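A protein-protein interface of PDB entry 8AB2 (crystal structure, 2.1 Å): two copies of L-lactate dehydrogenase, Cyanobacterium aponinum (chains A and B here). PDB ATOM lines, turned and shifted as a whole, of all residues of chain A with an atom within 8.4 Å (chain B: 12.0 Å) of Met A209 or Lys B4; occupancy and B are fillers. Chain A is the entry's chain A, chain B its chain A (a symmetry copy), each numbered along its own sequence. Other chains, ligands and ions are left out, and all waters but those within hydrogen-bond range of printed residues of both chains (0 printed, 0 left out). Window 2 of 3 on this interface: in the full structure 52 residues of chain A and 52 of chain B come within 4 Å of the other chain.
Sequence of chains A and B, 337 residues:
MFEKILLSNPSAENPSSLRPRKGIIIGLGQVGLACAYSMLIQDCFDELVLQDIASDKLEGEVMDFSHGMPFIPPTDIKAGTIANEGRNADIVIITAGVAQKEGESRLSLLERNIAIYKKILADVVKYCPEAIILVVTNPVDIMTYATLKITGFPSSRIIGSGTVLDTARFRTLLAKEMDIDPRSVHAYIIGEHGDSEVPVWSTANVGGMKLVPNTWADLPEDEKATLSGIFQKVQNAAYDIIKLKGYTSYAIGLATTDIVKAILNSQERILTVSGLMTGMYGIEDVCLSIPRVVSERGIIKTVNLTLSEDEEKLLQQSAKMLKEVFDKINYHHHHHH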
ATOM      1  N   MET A 178      -5.291  10.933  -0.427  1.00  0.00           N
ATOM      2  CA  MET A 178      -3.957  11.484  -0.234  1.00  0.00           C
ATOM      3  C   MET A 178      -2.868  10.676  -0.925  1.00  0.00           C
ATOM      4  O   MET A 178      -1.688  11.011  -0.781  1.00  0.00           O
ATOM      5  CB  MET A 178      -3.656  11.600   1.262  1.00  0.00           C
ATOM      6  CG  MET A 178      -4.717  12.382   2.025  1.00  0.00           C
ATOM      7  SD  MET A 178      -4.284  12.689   3.744  1.00  0.00           S
ATOM      8  CE  MET A 178      -2.801  13.670   3.544  1.00  0.00           C
ATOM      9  N   ILE A 180      -1.677   7.550  -0.434  1.00  0.00           N
ATOM     10  CA  ILE A 180      -0.777   7.022   0.583  1.00  0.00           C
ATOM     11  C   ILE A 180      -1.281   5.664   1.056  1.00  0.00           C
ATOM     12  O   ILE A 180      -2.472   5.354   0.970  1.00  0.00           O
ATOM     13  CB  ILE A 180      -0.630   8.007   1.769  1.00  0.00           C
ATOM     14  CG1 ILE A 180       0.605   7.672   2.610  1.00  0.00           C
ATOM     15  CG2 ILE A 180      -1.887   8.012   2.627  1.00  0.00           C
ATOM     16  CD1 ILE A 180       0.925   8.708   3.668  1.00  0.00           C
ATOM     17  N   SER A 184      -0.951   3.929   7.043  1.00  0.00           N
ATOM     18  CA  SER A 184      -0.386   5.142   7.616  1.00  0.00           C
ATOM     19  C   SER A 184      -1.444   6.054   8.224  1.00  0.00           C
ATOM     20  O   SER A 184      -1.093   7.078   8.817  1.00  0.00           O
ATOM     21  CB  SER A 184       0.397   5.914   6.550  1.00  0.00           C
ATOM     22  OG  SER A 184      -0.478   6.483   5.591  1.00  0.00           O
ATOM     23  N   VAL A 185      -2.721   5.706   8.093  1.00  0.00           N
ATOM     24  CA  VAL A 185      -3.827   6.543   8.541  1.00  0.00           C
ATOM     25  C   VAL A 185      -4.448   5.915   9.778  1.00  0.00           C
ATOM     26  O   VAL A 185      -4.779   4.722   9.780  1.00  0.00           O
ATOM     27  CB  VAL A 185      -4.880   6.723   7.434  1.00  0.00           C
ATOM     28  CG1 VAL A 185      -6.042   7.566   7.940  1.00  0.00           C
ATOM     29  CG2 VAL A 185      -4.252   7.351   6.201  1.00  0.00           C
ATOM     30  N   HIS A 186      -4.608   6.715  10.828  1.00  0.00           N
ATOM     31  CA  HIS A 186      -5.341   6.325  12.029  1.00  0.00           C
ATOM     32  C   HIS A 186      -6.505   7.297  12.183  1.00  0.00           C
ATOM     33  O   HIS A 186      -6.362   8.371  12.772  1.00  0.00           O
ATOM     34  CB  HIS A 186      -4.440   6.316  13.262  1.00  0.00           C
ATOM     35  CG  HIS A 186      -3.572   5.102  13.363  1.00  0.00           C
ATOM     36  ND1 HIS A 186      -2.249   5.097  12.977  1.00  0.00           N
ATOM     37  CD2 HIS A 186      -3.841   3.850  13.801  1.00  0.00           C
ATOM     38  CE1 HIS A 186      -1.740   3.894  13.176  1.00  0.00           C
ATOM     39  NE2 HIS A 186      -2.685   3.118  13.675  1.00  0.00           N
ATOM     40  N   SER A 202     -10.803  15.096  15.372  1.00  0.00           N
ATOM     41  CA  SER A 202      -9.845  15.830  16.193  1.00  0.00           C
ATOM     42  C   SER A 202      -8.515  15.095  16.313  1.00  0.00           C
ATOM     43  O   SER A 202      -7.466  15.734  16.452  1.00  0.00           O
ATOM     44  CB  SER A 202     -10.430  16.089  17.581  1.00  0.00           C
ATOM     45  OG  SER A 202     -10.662  14.871  18.271  1.00  0.00           O
ATOM     46  N   THR A 203      -8.534  13.765  16.264  1.00  0.00           N
ATOM     47  CA  THR A 203      -7.323  12.967  16.408  1.00  0.00           C
ATOM     48  C   THR A 203      -6.951  12.227  15.129  1.00  0.00           C
ATOM     49  O   THR A 203      -6.004  11.434  15.143  1.00  0.00           O
ATOM     50  CB  THR A 203      -7.473  11.969  17.558  1.00  0.00           C
ATOM     51  OG1 THR A 203      -8.360  10.914  17.165  1.00  0.00           O
ATOM     52  CG2 THR A 203      -8.032  12.659  18.792  1.00  0.00           C
ATOM     53  N   ALA A 204      -7.677  12.457  14.034  1.00  0.00           N
ATOM     54  CA  ALA A 204      -7.359  11.808  12.769  1.00  0.00           C
ATOM     55  C   ALA A 204      -5.922  12.111  12.370  1.00  0.00           C
ATOM     56  O   ALA A 204      -5.499  13.272  12.356  1.00  0.00           O
ATOM     57  CB  ALA A 204      -8.326  12.267  11.678  1.00  0.00           C
ATOM     58  N   ASN A 205      -5.168  11.062  12.055  1.00  0.00           N
ATOM     59  CA  ASN A 205      -3.724  11.160  11.909  1.00  0.00           C
ATOM     60  C   ASN A 205      -3.271  10.437  10.649  1.00  0.00           C
ATOM     61  O   ASN A 205      -3.776   9.357  10.325  1.00  0.00           O
ATOM     62  CB  ASN A 205      -3.021  10.573  13.138  1.00  0.00           C
ATOM     63  CG  ASN A 205      -1.537  10.855  13.150  1.00  0.00           C
ATOM     64  OD1 ASN A 205      -0.758  10.163  12.496  1.00  0.00           O
ATOM     65  ND2 ASN A 205      -1.135  11.873  13.903  1.00  0.00           N
ATOM     66  N   VAL A 206      -2.312  11.038   9.945  1.00  0.00           N
ATOM     67  CA  VAL A 206      -1.738  10.478   8.724  1.00  0.00           C
ATOM     68  C   VAL A 206      -0.225  10.466   8.880  1.00  0.00           C
ATOM     69  O   VAL A 206       0.418  11.518   8.791  1.00  0.00           O
ATOM     70  CB  VAL A 206      -2.143  11.266   7.473  1.00  0.00           C
ATOM     71  CG1 VAL A 206      -1.478  10.672   6.237  1.00  0.00           C
ATOM     72  CG2 VAL A 206      -3.658  11.277   7.315  1.00  0.00           C
ATOM     73  N   GLY A 207       0.341   9.282   9.114  1.00  0.00           N
ATOM     74  CA  GLY A 207       1.784   9.135   9.224  1.00  0.00           C
ATOM     75  C   GLY A 207       2.426   9.991  10.293  1.00  0.00           C
ATOM     76  O   GLY A 207       3.589  10.385  10.147  1.00  0.00           O
ATOM     77  N   GLY A 208       1.702  10.290  11.370  1.00  0.00           N
ATOM     78  CA  GLY A 208       2.179  11.166  12.415  1.00  0.00           C
ATOM     79  C   GLY A 208       1.601  12.565  12.367  1.00  0.00           C
ATOM     80  O   GLY A 208       1.556  13.238  13.404  1.00  0.00           O
ATOM     81  N   MET A 209       1.153  13.013  11.198  1.00  0.00           N
ATOM     82  CA  MET A 209       0.595  14.346  11.029  1.00  0.00           C
ATOM     83  C   MET A 209      -0.891  14.347  11.356  1.00  0.00           C
ATOM     84  O   MET A 209      -1.619  13.417  10.997  1.00  0.00           O
ATOM     85  CB  MET A 209       0.804  14.836   9.594  1.00  0.00           C
ATOM     86  CG  MET A 209       2.247  14.828   9.129  1.00  0.00           C
ATOM     87  SD  MET A 209       3.234  16.084   9.956  1.00  0.00           S
ATOM     88  CE  MET A 209       2.243  17.544   9.638  1.00  0.00           C
ATOM     89  N   LYS A 210      -1.340  15.401  12.031  1.00  0.00           N
ATOM     90  CA  LYS A 210      -2.757  15.566  12.317  1.00  0.00           C
ATOM     91  C   LYS A 210      -3.472  16.119  11.090  1.00  0.00           C
ATOM     92  O   LYS A 210      -3.048  17.128  10.519  1.00  0.00           O
ATOM     93  CB  LYS A 210      -2.960  16.500  13.511  1.00  0.00           C
ATOM     94  CG  LYS A 210      -2.329  16.011  14.805  1.00  0.00           C
ATOM     95  CD  LYS A 210      -2.561  16.994  15.943  1.00  0.00           C
ATOM     96  CE  LYS A 210      -4.042  17.156  16.247  1.00  0.00           C
ATOM     97  NZ  LYS A 210      -4.276  18.098  17.378  1.00  0.00           N
ATOM     98  N   LEU A 211      -4.551  15.446  10.677  1.00  0.00           N
ATOM     99  CA  LEU A 211      -5.389  15.991   9.614  1.00  0.00           C
ATOM    100  C   LEU A 211      -5.972  17.339  10.008  1.00  0.00           C
ATOM    101  O   LEU A 211      -6.145  18.218   9.156  1.00  0.00           O
ATOM    102  CB  LEU A 211      -6.513  15.014   9.269  1.00  0.00           C
ATOM    103  CG  LEU A 211      -6.274  14.065   8.095  1.00  0.00           C
ATOM    104  CD1 LEU A 211      -7.490  13.179   7.878  1.00  0.00           C
ATOM    105  CD2 LEU A 211      -5.950  14.853   6.836  1.00  0.00           C
ATOM    106  N   VAL A 212      -6.280  17.517  11.288  1.00  0.00           N
ATOM    107  CA  VAL A 212      -6.765  18.787  11.817  1.00  0.00           C
ATOM    108  C   VAL A 212      -5.693  19.328  12.754  1.00  0.00           C
ATOM    109  O   VAL A 212      -5.722  19.042  13.960  1.00  0.00           O
ATOM    110  CB  VAL A 212      -8.114  18.611  12.531  1.00  0.00           C
ATOM    111  CG1 VAL A 212      -8.676  19.957  12.939  1.00  0.00           C
ATOM    112  CG2 VAL A 212      -9.096  17.868  11.635  1.00  0.00           C
ATOM    113  N   PRO A 213      -4.728  20.102  12.249  1.00  0.00           N
ATOM    114  CA  PRO A 213      -3.600  20.516  13.101  1.00  0.00           C
ATOM    115  C   PRO A 213      -4.008  21.371  14.289  1.00  0.00           C
ATOM    116  O   PRO A 213      -3.376  21.281  15.349  1.00  0.00           O
ATOM    117  CB  PRO A 213      -2.696  21.290  12.130  1.00  0.00           C
ATOM    118  CG  PRO A 213      -3.606  21.728  11.026  1.00  0.00           C
ATOM    119  CD  PRO A 213      -4.617  20.632  10.880  1.00  0.00           C
ATOM    120  N   LEU A 219      -9.548  24.848   9.539  1.00  0.00           N
ATOM    121  CA  LEU A 219      -9.230  24.197   8.279  1.00  0.00           C
ATOM    122  C   LEU A 219      -9.722  25.034   7.099  1.00  0.00           C
ATOM    123  O   LEU A 219     -10.749  25.711   7.193  1.00  0.00           O
ATOM    124  CB  LEU A 219      -9.863  22.809   8.213  1.00  0.00           C
ATOM    125  CG  LEU A 219      -9.204  21.659   8.973  1.00  0.00           C
ATOM    126  CD1 LEU A 219     -10.032  20.394   8.817  1.00  0.00           C
ATOM    127  CD2 LEU A 219      -7.787  21.436   8.474  1.00  0.00           C
ATOM    128  N   PRO A 220      -9.001  25.007   5.979  1.00  0.00           N
ATOM    129  CA  PRO A 220      -9.502  25.663   4.767  1.00  0.00           C
ATOM    130  C   PRO A 220     -10.856  25.099   4.361  1.00  0.00           C
ATOM    131  O   PRO A 220     -11.190  23.951   4.660  1.00  0.00           O
ATOM    132  CB  PRO A 220      -8.426  25.349   3.721  1.00  0.00           C
ATOM    133  CG  PRO A 220      -7.188  25.113   4.522  1.00  0.00           C
ATOM    134  CD  PRO A 220      -7.647  24.457   5.793  1.00  0.00           C
ATOM    135  N   GLU A 223     -10.880  21.863   2.230  1.00  0.00           N
ATOM    136  CA  GLU A 223     -10.524  20.663   2.980  1.00  0.00           C
ATOM    137  C   GLU A 223     -11.676  20.208   3.867  1.00  0.00           C
ATOM    138  O   GLU A 223     -11.893  19.003   4.039  1.00  0.00           O
ATOM    139  CB  GLU A 223      -9.266  20.909   3.812  1.00  0.00           C
ATOM    140  CG  GLU A 223      -7.998  21.040   2.984  1.00  0.00           C
ATOM    141  CD  GLU A 223      -6.747  21.128   3.837  1.00  0.00           C
ATOM    142  OE1 GLU A 223      -6.871  21.137   5.080  1.00  0.00           O
ATOM    143  OE2 GLU A 223      -5.640  21.185   3.263  1.00  0.00           O
ATOM    144  N   MET B   1      -4.869  20.184  -2.210  1.00  0.00           N
ATOM    145  CA  MET B   1      -4.930  20.373  -0.765  1.00  0.00           C
ATOM    146  C   MET B   1      -4.115  19.312  -0.033  1.00  0.00           C
ATOM    147  O   MET B   1      -3.522  18.430  -0.659  1.00  0.00           O
ATOM    148  CB  MET B   1      -6.380  20.349  -0.284  1.00  0.00           C
ATOM    149  CG  MET B   1      -7.164  19.148  -0.774  1.00  0.00           C
ATOM    150  SD  MET B   1      -8.946  19.384  -0.665  1.00  0.00           S
ATOM    151  CE  MET B   1      -9.470  18.463  -2.108  1.00  0.00           C
ATOM    152  N   PHE B   2      -4.088  19.419   1.296  1.00  0.00           N
ATOM    153  CA  PHE B   2      -3.349  18.517   2.179  1.00  0.00           C
ATOM    154  C   PHE B   2      -1.840  18.600   1.967  1.00  0.00           C
ATOM    155  O   PHE B   2      -1.101  17.709   2.400  1.00  0.00           O
ATOM    156  CB  PHE B   2      -3.827  17.067   2.026  1.00  0.00           C
ATOM    157  CG  PHE B   2      -5.291  16.882   2.305  1.00  0.00           C
ATOM    158  CD1 PHE B   2      -5.867  17.419   3.444  1.00  0.00           C
ATOM    159  CD2 PHE B   2      -6.094  16.185   1.418  1.00  0.00           C
ATOM    160  CE1 PHE B   2      -7.216  17.254   3.700  1.00  0.00           C
ATOM    161  CE2 PHE B   2      -7.444  16.018   1.667  1.00  0.00           C
ATOM    162  CZ  PHE B   2      -8.005  16.553   2.810  1.00  0.00           C
ATOM    163  N   GLU B   3      -1.357  19.655   1.306  1.00  0.00           N
ATOM    164  CA  GLU B   3       0.078  19.822   1.122  1.00  0.00           C
ATOM    165  C   GLU B   3       0.801  20.151   2.420  1.00  0.00           C
ATOM    166  O   GLU B   3       2.034  20.073   2.459  1.00  0.00           O
ATOM    167  CB  GLU B   3       0.354  20.905   0.076  1.00  0.00           C
ATOM    168  CG  GLU B   3      -0.036  20.506  -1.343  1.00  0.00           C
ATOM    169  CD  GLU B   3       0.833  19.392  -1.903  1.00  0.00           C
ATOM    170  OE1 GLU B   3       2.073  19.483  -1.786  1.00  0.00           O
ATOM    171  OE2 GLU B   3       0.275  18.421  -2.455  1.00  0.00           O
ATOM    172  N   LYS B   4       0.073  20.516   3.478  1.00  0.00           N
ATOM    173  CA  LYS B   4       0.668  20.675   4.797  1.00  0.00           C
ATOM    174  C   LYS B   4       0.883  19.340   5.495  1.00  0.00           C
ATOM    175  O   LYS B   4       1.559  19.301   6.529  1.00  0.00           O
ATOM    176  CB  LYS B   4      -0.211  21.579   5.665  1.00  0.00           C
ATOM    177  N   ILE B   5       0.325  18.256   4.959  1.00  0.00           N
ATOM    178  CA  ILE B   5       0.538  16.914   5.485  1.00  0.00           C
ATOM    179  C   ILE B   5       1.573  16.211   4.618  1.00  0.00           C
ATOM    180  O   ILE B   5       2.605  15.743   5.113  1.00  0.00           O
ATOM    181  CB  ILE B   5      -0.776  16.110   5.527  1.00  0.00           C
ATOM    182  CG1 ILE B   5      -1.878  16.916   6.218  1.00  0.00           C
ATOM    183  CG2 ILE B   5      -0.562  14.779   6.229  1.00  0.00           C
ATOM    184  CD1 ILE B   5      -1.575  17.249   7.654  1.00  0.00           C
ATOM    185  N   LEU B   6       1.301  16.137   3.316  1.00  0.00           N
ATOM    186  CA  LEU B   6       2.169  15.465   2.356  1.00  0.00           C
ATOM    187  C   LEU B   6       2.572  16.462   1.281  1.00  0.00           C
ATOM    188  O   LEU B   6       1.718  16.971   0.548  1.00  0.00           O
ATOM    189  CB  LEU B   6       1.465  14.258   1.732  1.00  0.00           C
ATOM    190  CG  LEU B   6       0.880  13.236   2.707  1.00  0.00           C
ATOM    191  CD1 LEU B   6       0.233  12.085   1.952  1.00  0.00           C
ATOM    192  CD2 LEU B   6       1.951  12.725   3.660  1.00  0.00           C
ATOM    193  N   LEU B   7       3.869  16.737   1.188  1.00  0.00           N
ATOM    194  CA  LEU B   7       4.398  17.684   0.216  1.00  0.00           C
ATOM    195  C   LEU B   7       4.790  16.931  -1.050  1.00  0.00           C
ATOM    196  O   LEU B   7       5.690  16.085  -1.021  1.00  0.00           O
ATOM    197  CB  LEU B   7       5.597  18.433   0.799  1.00  0.00           C
ATOM    198  CG  LEU B   7       6.091  19.675   0.059  1.00  0.00           C
ATOM    199  CD1 LEU B   7       5.008  20.742   0.019  1.00  0.00           C
ATOM    200  CD2 LEU B   7       7.351  20.213   0.717  1.00  0.00           C
ATOM    201  N   SER B   8       4.114  17.237  -2.155  1.00  0.00           N
ATOM    202  CA  SER B   8       4.383  16.549  -3.410  1.00  0.00           C
ATOM    203  C   SER B   8       5.765  16.910  -3.940  1.00  0.00           C
ATOM    204  O   SER B   8       6.195  18.065  -3.868  1.00  0.00           O
ATOM    205  CB  SER B   8       3.316  16.898  -4.447  1.00  0.00           C
ATOM    206  OG  SER B   8       2.045  16.412  -4.054  1.00  0.00           O
ATOM    207  N   ASN B   9       6.462  15.909  -4.473  1.00  0.00           N
ATOM    208  CA  ASN B   9       7.794  16.110  -5.028  1.00  0.00           C
ATOM    209  C   ASN B   9       7.676  16.557  -6.478  1.00  0.00           C
ATOM    210  O   ASN B   9       7.107  15.819  -7.295  1.00  0.00           O
ATOM    211  CB  ASN B   9       8.609  14.830  -4.936  1.00  0.00           C
ATOM    212  CG  ASN B   9      10.077  15.045  -5.257  1.00  0.00           C
ATOM    213  OD1 ASN B   9      10.553  16.178  -5.320  1.00  0.00           O
ATOM    214  ND2 ASN B   9      10.803  13.952  -5.452  1.00  0.00           N
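Printed residues of chain B within 4 Å of Met A178: Phe B2 (3.9 Å), Ile B5 (3.7 Å) and Leu B6 (3.5 Å). Of the printed residues of chain B, Ile A180 touches Leu B6. No residue of chain B comes within 4 Å of Ala A204. No residue of chain B comes within 4 Å of Asn A205. Gly A208 touches none of the printed residues of chain B. Of chain B, only Lys B4 and Ile B5 come within 4 Å of Met A209. Lys A210 touches just one residue of chain B: Ile B5. No residue of chain B comes within 4 Å of Leu A211. Of the printed residues of chain B, Glu A223 touches Met B1 (3.7 Å) and Phe B2 (3.1 Å). Of the printed residues of chain A, Met B1 touches Glu A223 (3.7 Å). Of the printed residues of chain A, Phe B2 touches Met A178 (3.9 Å) and Glu A223 (3.1 Å). Printed residues of chain A within 4 Å of Lys B4: Met A209. Ile B5 touches just these residues of chain A: Met A178 (3.7 Å), Met A209 (3.6 Å) and Lys A210 (3.2 Å). The nearest residue of chain B that does not touch Met A209 is Leu B6 (5.9 Å). The nearest residue of chain A that does not touch Lys B4 is Glu A223 (5.8 Å).
OE2 of Glu A223 sits at hydrogen-bond distance from N of Phe B2, 3.1 Å away.
No position is printed for both chains. Of the 9 pairs that touch across the chains among the printed residues, none has its exchanged pair printed and touching as well.
The backbone carbonyl oxygen (O) of Met A209 sits close to the side-chain amide nitrogen (ND2) of Asn A205 (3.3 Å).
Hydrophobic or aromatic side chains of chain B within 4 Å of the printed part of chain A: Met B1, Phe B2, Ile B5 and Leu B6. Of the 20 printed residues of chain A, 5 touch a printed residue of chain B. Hydrophobic or aromatic side chains of chain A within 4 Å of the printed part of chain B: Met A178, Ile A180 and Met A209. Among the printed residues, no Asp or Glu carboxylate lies within 4 Å of a Lys or Arg side-chain nitrogen of the other chain.
Among the printed residues, merely in contact across the chains: Lys A210 with Ile B5 (3.2 Å), Met A178 with Leu B6 (3.5 Å), Met A209 with Ile B5 (3.6 Å), Met A209 with Lys B4 (3.6 Å), Met A178 with Ile B5 (3.7 Å), Glu A223 with Met B1 (3.7 Å), Ile A180 with Leu B6 (3.9 Å) and Met A178 with Phe B2 (3.9 Å).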
